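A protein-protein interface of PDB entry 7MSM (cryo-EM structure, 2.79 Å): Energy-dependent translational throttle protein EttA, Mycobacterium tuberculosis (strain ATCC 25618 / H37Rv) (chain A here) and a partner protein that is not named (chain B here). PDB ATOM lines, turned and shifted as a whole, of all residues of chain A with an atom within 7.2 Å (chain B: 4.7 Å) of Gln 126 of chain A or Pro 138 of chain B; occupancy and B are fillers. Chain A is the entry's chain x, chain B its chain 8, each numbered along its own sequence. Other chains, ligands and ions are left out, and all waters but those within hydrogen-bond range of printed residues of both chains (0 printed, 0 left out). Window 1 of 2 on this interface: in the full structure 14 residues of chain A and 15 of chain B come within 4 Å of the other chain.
Of chain B, only Met 137 and Pro 138 come within 4 Å of Gln 126 of chain A. Of the printed residues of chain B, Glu 127 of chain A touches Asn 139. Of the printed residues of chain A, Ala 128 of chain B touches Trp 135. Printed residues of chain A within 4 Å of Met 137 of chain B: Gln 126 (3.4 Å). Pro 138 of chain B touches just one residue of chain A: Gln 126. Printed residues of chain A within 4 Å of Asn 139 of chain B: Glu 127. Printed residues of chain A within 4 Å of Val 145 of chain B: Met 119 (3.3 Å). The nearest residue of chain A that does not touch Pro 138 of chain B is Met 122 of chain A (5.4 Å). The nearest printed residue of chain A that does not touch Pro 140 of chain B is Gly 123 of chain A (4.3 Å).
The side-chain carboxylate (OE2) of Glu 127 of chain A lies close to the side-chain amide oxygen (OD1) of Asn 139 of chain B (2.9 Å). SD of Met 119 of chain A lies close to O of Val 145 of chain B (3.3 Å).
The indole nitrogen (NE1) of Trp 135 of chain A lies within hydrogen-bond range of the backbone carbonyl oxygen (O) of Leu 129 of chain A, 2.7 Å away. The side-chain hydroxyl of Thr 144 of chain B is in hydrogen-bond range of the backbone carbonyl oxygen of Asn 139 of chain B, 2.4 Å away. The backbone carbonyl oxygen of Asn 139 of chain B lies within hydrogen-bond range of the backbone NH of Val 145 of chain B (3.3 Å).
Among the printed residues, merely in contact across the chains: Gln 126 of chain A with Met 137 of chain B (3.4 Å), Met 119 of chain A with Pro 140 of chain B (3.4 Å), Trp 135 of chain A with Ala 128 of chain B (3.9 Å) and Gln 126 of chain A with Pro 138 of chain B (3.9 Å).
Of the 16 printed residues of chain A, 4 touch a printed residue of chain B. Hydrophobic or aromatic side chains of chain A that line the printed part of chain B: Met 119 and Trp 135. Printed residues of chain B that touch a printed residue of chain A: Ala 128, Met 137, Pro 138, Asn 139, Pro 140 and Val 145. Hydrophobic or aromatic side chains of chain B that line the printed part of chain A: Ala 128, Met 137, Pro 140 and Val 145.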
ATOM      1  N   LYS A  99       2.847 -31.045 -11.488  1.00  0.00           N
ATOM      2  CA  LYS A  99       3.220 -30.273 -12.664  1.00  0.00           C
ATOM      3  C   LYS A  99       3.155 -31.112 -13.931  1.00  0.00           C
ATOM      4  O   LYS A  99       3.132 -30.552 -15.031  1.00  0.00           O
ATOM      5  CB  LYS A  99       4.622 -29.676 -12.500  1.00  0.00           C
ATOM      6  CG  LYS A  99       4.665 -28.317 -11.808  1.00  0.00           C
ATOM      7  CD  LYS A  99       4.471 -28.394 -10.306  1.00  0.00           C
ATOM      8  CE  LYS A  99       4.608 -27.024  -9.667  1.00  0.00           C
ATOM      9  NZ  LYS A  99       4.318 -27.068  -8.207  1.00  0.00           N
ATOM     10  N   PHE A 103       0.056 -30.782 -17.052  1.00  0.00           N
ATOM     11  CA  PHE A 103       0.468 -30.747 -18.452  1.00  0.00           C
ATOM     12  C   PHE A 103      -0.336 -31.726 -19.299  1.00  0.00           C
ATOM     13  O   PHE A 103      -0.619 -31.450 -20.469  1.00  0.00           O
ATOM     14  CB  PHE A 103       1.961 -31.048 -18.572  1.00  0.00           C
ATOM     15  CG  PHE A 103       2.484 -30.969 -19.977  1.00  0.00           C
ATOM     16  CD1 PHE A 103       2.754 -29.742 -20.557  1.00  0.00           C
ATOM     17  CD2 PHE A 103       2.693 -32.121 -20.723  1.00  0.00           C
ATOM     18  CE1 PHE A 103       3.230 -29.661 -21.853  1.00  0.00           C
ATOM     19  CE2 PHE A 103       3.162 -32.048 -22.020  1.00  0.00           C
ATOM     20  CZ  PHE A 103       3.434 -30.817 -22.585  1.00  0.00           C
ATOM     21  N   MET A 119      -1.671 -20.020 -22.579  1.00  0.00           N
ATOM     22  CA  MET A 119      -0.424 -20.200 -23.313  1.00  0.00           C
ATOM     23  C   MET A 119       0.782 -20.136 -22.386  1.00  0.00           C
ATOM     24  O   MET A 119       1.741 -20.900 -22.550  1.00  0.00           O
ATOM     25  CB  MET A 119      -0.323 -19.137 -24.406  1.00  0.00           C
ATOM     26  CG  MET A 119       0.878 -19.259 -25.311  1.00  0.00           C
ATOM     27  SD  MET A 119       0.885 -17.957 -26.556  1.00  0.00           S
ATOM     28  CE  MET A 119      -0.452 -18.494 -27.619  1.00  0.00           C
ATOM     29  N   GLU A 120       0.753 -19.237 -21.405  1.00  0.00           N
ATOM     30  CA  GLU A 120       1.808 -19.178 -20.405  1.00  0.00           C
ATOM     31  C   GLU A 120       1.549 -20.097 -19.218  1.00  0.00           C
ATOM     32  O   GLU A 120       2.490 -20.413 -18.483  1.00  0.00           O
ATOM     33  CB  GLU A 120       2.004 -17.730 -19.932  1.00  0.00           C
ATOM     34  CG  GLU A 120       0.763 -17.048 -19.364  1.00  0.00           C
ATOM     35  CD  GLU A 120       0.620 -17.217 -17.864  1.00  0.00           C
ATOM     36  OE1 GLU A 120       1.629 -17.538 -17.202  1.00  0.00           O
ATOM     37  OE2 GLU A 120      -0.499 -17.021 -17.350  1.00  0.00           O
ATOM     38  N   GLU A 121       0.300 -20.532 -19.021  1.00  0.00           N
ATOM     39  CA  GLU A 121      -0.001 -21.476 -17.949  1.00  0.00           C
ATOM     40  C   GLU A 121       0.599 -22.847 -18.223  1.00  0.00           C
ATOM     41  O   GLU A 121       0.989 -23.550 -17.285  1.00  0.00           O
ATOM     42  CB  GLU A 121      -1.512 -21.586 -17.753  1.00  0.00           C
ATOM     43  CG  GLU A 121      -2.150 -20.329 -17.194  1.00  0.00           C
ATOM     44  CD  GLU A 121      -1.750 -20.064 -15.756  1.00  0.00           C
ATOM     45  OE1 GLU A 121      -1.521 -21.038 -15.008  1.00  0.00           O
ATOM     46  OE2 GLU A 121      -1.667 -18.879 -15.372  1.00  0.00           O
ATOM     47  N   MET A 122       0.675 -23.245 -19.490  1.00  0.00           N
ATOM     48  CA  MET A 122       1.479 -24.393 -19.868  1.00  0.00           C
ATOM     49  C   MET A 122       2.913 -24.006 -20.184  1.00  0.00           C
ATOM     50  O   MET A 122       3.763 -24.890 -20.327  1.00  0.00           O
ATOM     51  CB  MET A 122       0.844 -25.121 -21.064  1.00  0.00           C
ATOM     52  CG  MET A 122       0.728 -24.334 -22.368  1.00  0.00           C
ATOM     53  SD  MET A 122       2.159 -24.440 -23.469  1.00  0.00           S
ATOM     54  CE  MET A 122       2.064 -26.155 -23.973  1.00  0.00           C
ATOM     55  N   GLY A 123       3.198 -22.713 -20.296  1.00  0.00           N
ATOM     56  CA  GLY A 123       4.534 -22.250 -20.596  1.00  0.00           C
ATOM     57  C   GLY A 123       5.449 -22.321 -19.395  1.00  0.00           C
ATOM     58  O   GLY A 123       6.604 -22.740 -19.509  1.00  0.00           O
ATOM     59  N   ARG A 124       4.941 -21.921 -18.230  1.00  0.00           N
ATOM     60  CA  ARG A 124       5.721 -21.957 -17.000  1.00  0.00           C
ATOM     61  C   ARG A 124       5.723 -23.329 -16.340  1.00  0.00           C
ATOM     62  O   ARG A 124       6.258 -23.469 -15.236  1.00  0.00           O
ATOM     63  CB  ARG A 124       5.204 -20.900 -16.020  1.00  0.00           C
ATOM     64  CG  ARG A 124       3.790 -21.136 -15.533  1.00  0.00           C
ATOM     65  CD  ARG A 124       3.339 -20.016 -14.612  1.00  0.00           C
ATOM     66  NE  ARG A 124       1.943 -20.162 -14.211  1.00  0.00           N
ATOM     67  CZ  ARG A 124       1.540 -20.845 -13.145  1.00  0.00           C
ATOM     68  NH1 ARG A 124       2.427 -21.446 -12.364  1.00  0.00           N
ATOM     69  NH2 ARG A 124       0.248 -20.924 -12.858  1.00  0.00           N
ATOM     70  N   LEU A 125       5.140 -24.336 -16.982  1.00  0.00           N
ATOM     71  CA  LEU A 125       5.186 -25.703 -16.491  1.00  0.00           C
ATOM     72  C   LEU A 125       5.906 -26.657 -17.426  1.00  0.00           C
ATOM     73  O   LEU A 125       6.477 -27.641 -16.954  1.00  0.00           O
ATOM     74  CB  LEU A 125       3.767 -26.227 -16.236  1.00  0.00           C
ATOM     75  CG  LEU A 125       2.989 -25.417 -15.198  1.00  0.00           C
ATOM     76  CD1 LEU A 125       1.585 -25.972 -15.010  1.00  0.00           C
ATOM     77  CD2 LEU A 125       3.738 -25.342 -13.876  1.00  0.00           C
ATOM     78  N   GLN A 126       5.896 -26.399 -18.735  1.00  0.00           N
ATOM     79  CA  GLN A 126       6.666 -27.231 -19.649  1.00  0.00           C
ATOM     80  C   GLN A 126       8.151 -26.909 -19.557  1.00  0.00           C
ATOM     81  O   GLN A 126       8.992 -27.776 -19.821  1.00  0.00           O
ATOM     82  CB  GLN A 126       6.156 -27.052 -21.081  1.00  0.00           C
ATOM     83  CG  GLN A 126       6.667 -28.081 -22.073  1.00  0.00           C
ATOM     84  CD  GLN A 126       6.073 -27.894 -23.452  1.00  0.00           C
ATOM     85  OE1 GLN A 126       5.335 -26.940 -23.698  1.00  0.00           O
ATOM     86  NE2 GLN A 126       6.380 -28.815 -24.359  1.00  0.00           N
ATOM     87  N   GLU A 127       8.491 -25.683 -19.161  1.00  0.00           N
ATOM     88  CA  GLU A 127       9.866 -25.334 -18.824  1.00  0.00           C
ATOM     89  C   GLU A 127      10.266 -25.792 -17.430  1.00  0.00           C
ATOM     90  O   GLU A 127      11.406 -25.553 -17.020  1.00  0.00           O
ATOM     91  CB  GLU A 127      10.085 -23.825 -18.944  1.00  0.00           C
ATOM     92  CG  GLU A 127      10.066 -23.305 -20.367  1.00  0.00           C
ATOM     93  CD  GLU A 127      10.351 -21.818 -20.448  1.00  0.00           C
ATOM     94  OE1 GLU A 127      10.434 -21.163 -19.388  1.00  0.00           O
ATOM     95  OE2 GLU A 127      10.504 -21.305 -21.575  1.00  0.00           O
ATOM     96  N   GLU A 128       9.357 -26.413 -16.681  1.00  0.00           N
ATOM     97  CA  GLU A 128       9.708 -27.114 -15.457  1.00  0.00           C
ATOM     98  C   GLU A 128       9.831 -28.613 -15.688  1.00  0.00           C
ATOM     99  O   GLU A 128       9.652 -29.399 -14.754  1.00  0.00           O
ATOM    100  CB  GLU A 128       8.688 -26.817 -14.360  1.00  0.00           C
ATOM    101  CG  GLU A 128       8.712 -25.372 -13.889  1.00  0.00           C
ATOM    102  CD  GLU A 128       7.711 -25.102 -12.788  1.00  0.00           C
ATOM    103  OE1 GLU A 128       6.923 -26.014 -12.468  1.00  0.00           O
ATOM    104  OE2 GLU A 128       7.707 -23.978 -12.244  1.00  0.00           O
ATOM    105  N   LEU A 129      10.120 -29.018 -16.925  1.00  0.00           N
ATOM    106  CA  LEU A 129      10.277 -30.419 -17.284  1.00  0.00           C
ATOM    107  C   LEU A 129      11.516 -30.615 -18.146  1.00  0.00           C
ATOM    108  O   LEU A 129      11.572 -31.546 -18.953  1.00  0.00           O
ATOM    109  CB  LEU A 129       9.049 -30.949 -18.030  1.00  0.00           C
ATOM    110  CG  LEU A 129       7.689 -30.934 -17.329  1.00  0.00           C
ATOM    111  CD1 LEU A 129       6.595 -31.406 -18.273  1.00  0.00           C
ATOM    112  CD2 LEU A 129       7.705 -31.763 -16.065  1.00  0.00           C
ATOM    113  N   ASP A 130      12.500 -29.731 -18.017  1.00  0.00           N
ATOM    114  CA  ASP A 130      13.758 -29.908 -18.728  1.00  0.00           C
ATOM    115  C   ASP A 130      14.940 -29.714 -17.786  1.00  0.00           C
ATOM    116  O   ASP A 130      16.019 -30.268 -18.013  1.00  0.00           O
ATOM    117  CB  ASP A 130      13.839 -28.959 -19.931  1.00  0.00           C
ATOM    118  CG  ASP A 130      13.636 -27.496 -19.555  1.00  0.00           C
ATOM    119  OD1 ASP A 130      13.317 -27.203 -18.386  1.00  0.00           O
ATOM    120  OD2 ASP A 130      13.802 -26.631 -20.442  1.00  0.00           O
ATOM    121  N   HIS A 131      14.744 -28.931 -16.723  1.00  0.00           N
ATOM    122  CA  HIS A 131      15.783 -28.793 -15.716  1.00  0.00           C
ATOM    123  C   HIS A 131      15.854 -30.009 -14.808  1.00  0.00           C
ATOM    124  O   HIS A 131      16.911 -30.276 -14.227  1.00  0.00           O
ATOM    125  CB  HIS A 131      15.556 -27.540 -14.866  1.00  0.00           C
ATOM    126  CG  HIS A 131      14.427 -27.667 -13.894  1.00  0.00           C
ATOM    127  ND1 HIS A 131      13.105 -27.530 -14.261  1.00  0.00           N
ATOM    128  CD2 HIS A 131      14.424 -27.923 -12.565  1.00  0.00           C
ATOM    129  CE1 HIS A 131      12.338 -27.694 -13.197  1.00  0.00           C
ATOM    130  NE2 HIS A 131      13.113 -27.937 -12.157  1.00  0.00           N
ATOM    131  N   TRP A 135      10.255 -36.055 -17.600  1.00  0.00           N
ATOM    132  CA  TRP A 135       9.443 -36.790 -18.557  1.00  0.00           C
ATOM    133  C   TRP A 135       9.481 -38.289 -18.310  1.00  0.00           C
ATOM    134  O   TRP A 135       8.557 -38.997 -18.721  1.00  0.00           O
ATOM    135  CB  TRP A 135       9.912 -36.504 -19.984  1.00  0.00           C
ATOM    136  CG  TRP A 135       9.720 -35.085 -20.388  1.00  0.00           C
ATOM    137  CD1 TRP A 135      10.657 -34.100 -20.372  1.00  0.00           C
ATOM    138  CD2 TRP A 135       8.513 -34.485 -20.863  1.00  0.00           C
ATOM    139  NE1 TRP A 135      10.110 -32.917 -20.806  1.00  0.00           N
ATOM    140  CE2 TRP A 135       8.793 -33.129 -21.116  1.00  0.00           C
ATOM    141  CE3 TRP A 135       7.221 -34.963 -21.102  1.00  0.00           C
ATOM    142  CZ2 TRP A 135       7.833 -32.247 -21.597  1.00  0.00           C
ATOM    143  CZ3 TRP A 135       6.269 -34.086 -21.579  1.00  0.00           C
ATOM    144  CH2 TRP A 135       6.579 -32.743 -21.821  1.00  0.00           C
ATOM    145  N   ALA B 114      10.384 -25.877 -33.370  1.00  0.00           N
ATOM    146  CA  ALA B 114       8.977 -26.276 -33.337  1.00  0.00           C
ATOM    147  C   ALA B 114       8.136 -25.027 -33.093  1.00  0.00           C
ATOM    148  O   ALA B 114       8.003 -24.579 -31.950  1.00  0.00           O
ATOM    149  CB  ALA B 114       8.734 -27.330 -32.266  1.00  0.00           C
ATOM    150  N   ALA B 116       4.431 -23.786 -33.356  1.00  0.00           N
ATOM    151  CA  ALA B 116       3.100 -24.366 -33.447  1.00  0.00           C
ATOM    152  C   ALA B 116       2.031 -23.282 -33.362  1.00  0.00           C
ATOM    153  O   ALA B 116       2.318 -22.090 -33.212  1.00  0.00           O
ATOM    154  CB  ALA B 116       2.903 -25.417 -32.354  1.00  0.00           C
ATOM    155  N   VAL B 124       1.029 -31.634 -29.531  1.00  0.00           N
ATOM    156  CA  VAL B 124       2.345 -31.224 -29.054  1.00  0.00           C
ATOM    157  C   VAL B 124       2.738 -32.027 -27.819  1.00  0.00           C
ATOM    158  O   VAL B 124       3.890 -32.458 -27.682  1.00  0.00           O
ATOM    159  CB  VAL B 124       2.350 -29.706 -28.789  1.00  0.00           C
ATOM    160  CG1 VAL B 124       3.676 -29.249 -28.202  1.00  0.00           C
ATOM    161  CG2 VAL B 124       2.048 -28.952 -30.073  1.00  0.00           C
ATOM    162  N   ALA B 128       6.000 -34.482 -27.645  1.00  0.00           N
ATOM    163  CA  ALA B 128       7.050 -34.139 -26.693  1.00  0.00           C
ATOM    164  C   ALA B 128       7.494 -35.327 -25.845  1.00  0.00           C
ATOM    165  O   ALA B 128       8.176 -35.125 -24.835  1.00  0.00           O
ATOM    166  CB  ALA B 128       6.587 -33.000 -25.782  1.00  0.00           C
ATOM    167  N   LEU B 136      13.484 -29.440 -27.793  1.00  0.00           N
ATOM    168  CA  LEU B 136      12.878 -28.812 -28.961  1.00  0.00           C
ATOM    169  C   LEU B 136      11.386 -28.569 -28.765  1.00  0.00           C
ATOM    170  O   LEU B 136      10.610 -28.656 -29.721  1.00  0.00           O
ATOM    171  CB  LEU B 136      13.125 -29.649 -30.217  1.00  0.00           C
ATOM    172  CG  LEU B 136      14.474 -29.506 -30.939  1.00  0.00           C
ATOM    173  CD1 LEU B 136      15.616 -30.226 -30.235  1.00  0.00           C
ATOM    174  CD2 LEU B 136      14.362 -29.978 -32.377  1.00  0.00           C
ATOM    175  N   MET B 137      10.974 -28.281 -27.533  1.00  0.00           N
ATOM    176  CA  MET B 137       9.589 -27.958 -27.250  1.00  0.00           C
ATOM    177  C   MET B 137       9.219 -26.601 -27.844  1.00  0.00           C
ATOM    178  O   MET B 137      10.076 -25.731 -28.007  1.00  0.00           O
ATOM    179  CB  MET B 137       9.343 -27.964 -25.741  1.00  0.00           C
ATOM    180  CG  MET B 137      10.317 -27.123 -24.901  1.00  0.00           C
ATOM    181  SD  MET B 137      10.003 -25.345 -24.762  1.00  0.00           S
ATOM    182  CE  MET B 137       8.548 -25.320 -23.723  1.00  0.00           C
ATOM    183  N   PRO B 138       7.950 -26.405 -28.205  1.00  0.00           N
ATOM    184  CA  PRO B 138       7.500 -25.066 -28.613  1.00  0.00           C
ATOM    185  C   PRO B 138       7.392 -24.165 -27.392  1.00  0.00           C
ATOM    186  O   PRO B 138       6.679 -24.479 -26.437  1.00  0.00           O
ATOM    187  CB  PRO B 138       6.129 -25.332 -29.249  1.00  0.00           C
ATOM    188  CG  PRO B 138       6.141 -26.773 -29.604  1.00  0.00           C
ATOM    189  CD  PRO B 138       6.952 -27.435 -28.532  1.00  0.00           C
ATOM    190  N   ASN B 139       8.112 -23.044 -27.424  1.00  0.00           N
ATOM    191  CA  ASN B 139       8.187 -22.124 -26.296  1.00  0.00           C
ATOM    192  C   ASN B 139       7.378 -20.872 -26.594  1.00  0.00           C
ATOM    193  O   ASN B 139       7.595 -20.236 -27.635  1.00  0.00           O
ATOM    194  CB  ASN B 139       9.650 -21.751 -26.014  1.00  0.00           C
ATOM    195  CG  ASN B 139       9.842 -21.033 -24.682  1.00  0.00           C
ATOM    196  OD1 ASN B 139       8.892 -20.784 -23.940  1.00  0.00           O
ATOM    197  ND2 ASN B 139      11.091 -20.706 -24.373  1.00  0.00           N
ATOM    198  N   PRO B 140       6.433 -20.498 -25.725  1.00  0.00           N
ATOM    199  CA  PRO B 140       5.722 -19.226 -25.927  1.00  0.00           C
ATOM    200  C   PRO B 140       6.587 -17.998 -25.711  1.00  0.00           C
ATOM    201  O   PRO B 140       6.322 -16.961 -26.329  1.00  0.00           O
ATOM    202  CB  PRO B 140       4.586 -19.294 -24.899  1.00  0.00           C
ATOM    203  CG  PRO B 140       4.391 -20.743 -24.651  1.00  0.00           C
ATOM    204  CD  PRO B 140       5.758 -21.349 -24.732  1.00  0.00           C
ATOM    205  N   THR B 144       7.526 -18.917 -30.425  1.00  0.00           N
ATOM    206  CA  THR B 144       7.209 -20.087 -31.232  1.00  0.00           C
ATOM    207  C   THR B 144       5.788 -20.585 -31.008  1.00  0.00           C
ATOM    208  O   THR B 144       5.258 -21.310 -31.857  1.00  0.00           O
ATOM    209  CB  THR B 144       8.205 -21.211 -30.946  1.00  0.00           C
ATOM    210  OG1 THR B 144       8.095 -21.612 -29.577  1.00  0.00           O
ATOM    211  CG2 THR B 144       9.620 -20.731 -31.205  1.00  0.00           C
ATOM    212  N   VAL B 145       5.158 -20.215 -29.901  1.00  0.00           N
ATOM    213  CA  VAL B 145       3.750 -20.509 -29.669  1.00  0.00           C
ATOM    214  C   VAL B 145       3.004 -19.195 -29.844  1.00  0.00           C
ATOM    215  O   VAL B 145       3.039 -18.325 -28.966  1.00  0.00           O
ATOM    216  CB  VAL B 145       3.501 -21.113 -28.285  1.00  0.00           C
ATOM    217  CG1 VAL B 145       2.024 -21.424 -28.107  1.00  0.00           C
ATOM    218  CG2 VAL B 145       4.341 -22.347 -28.086  1.00  0.00           C
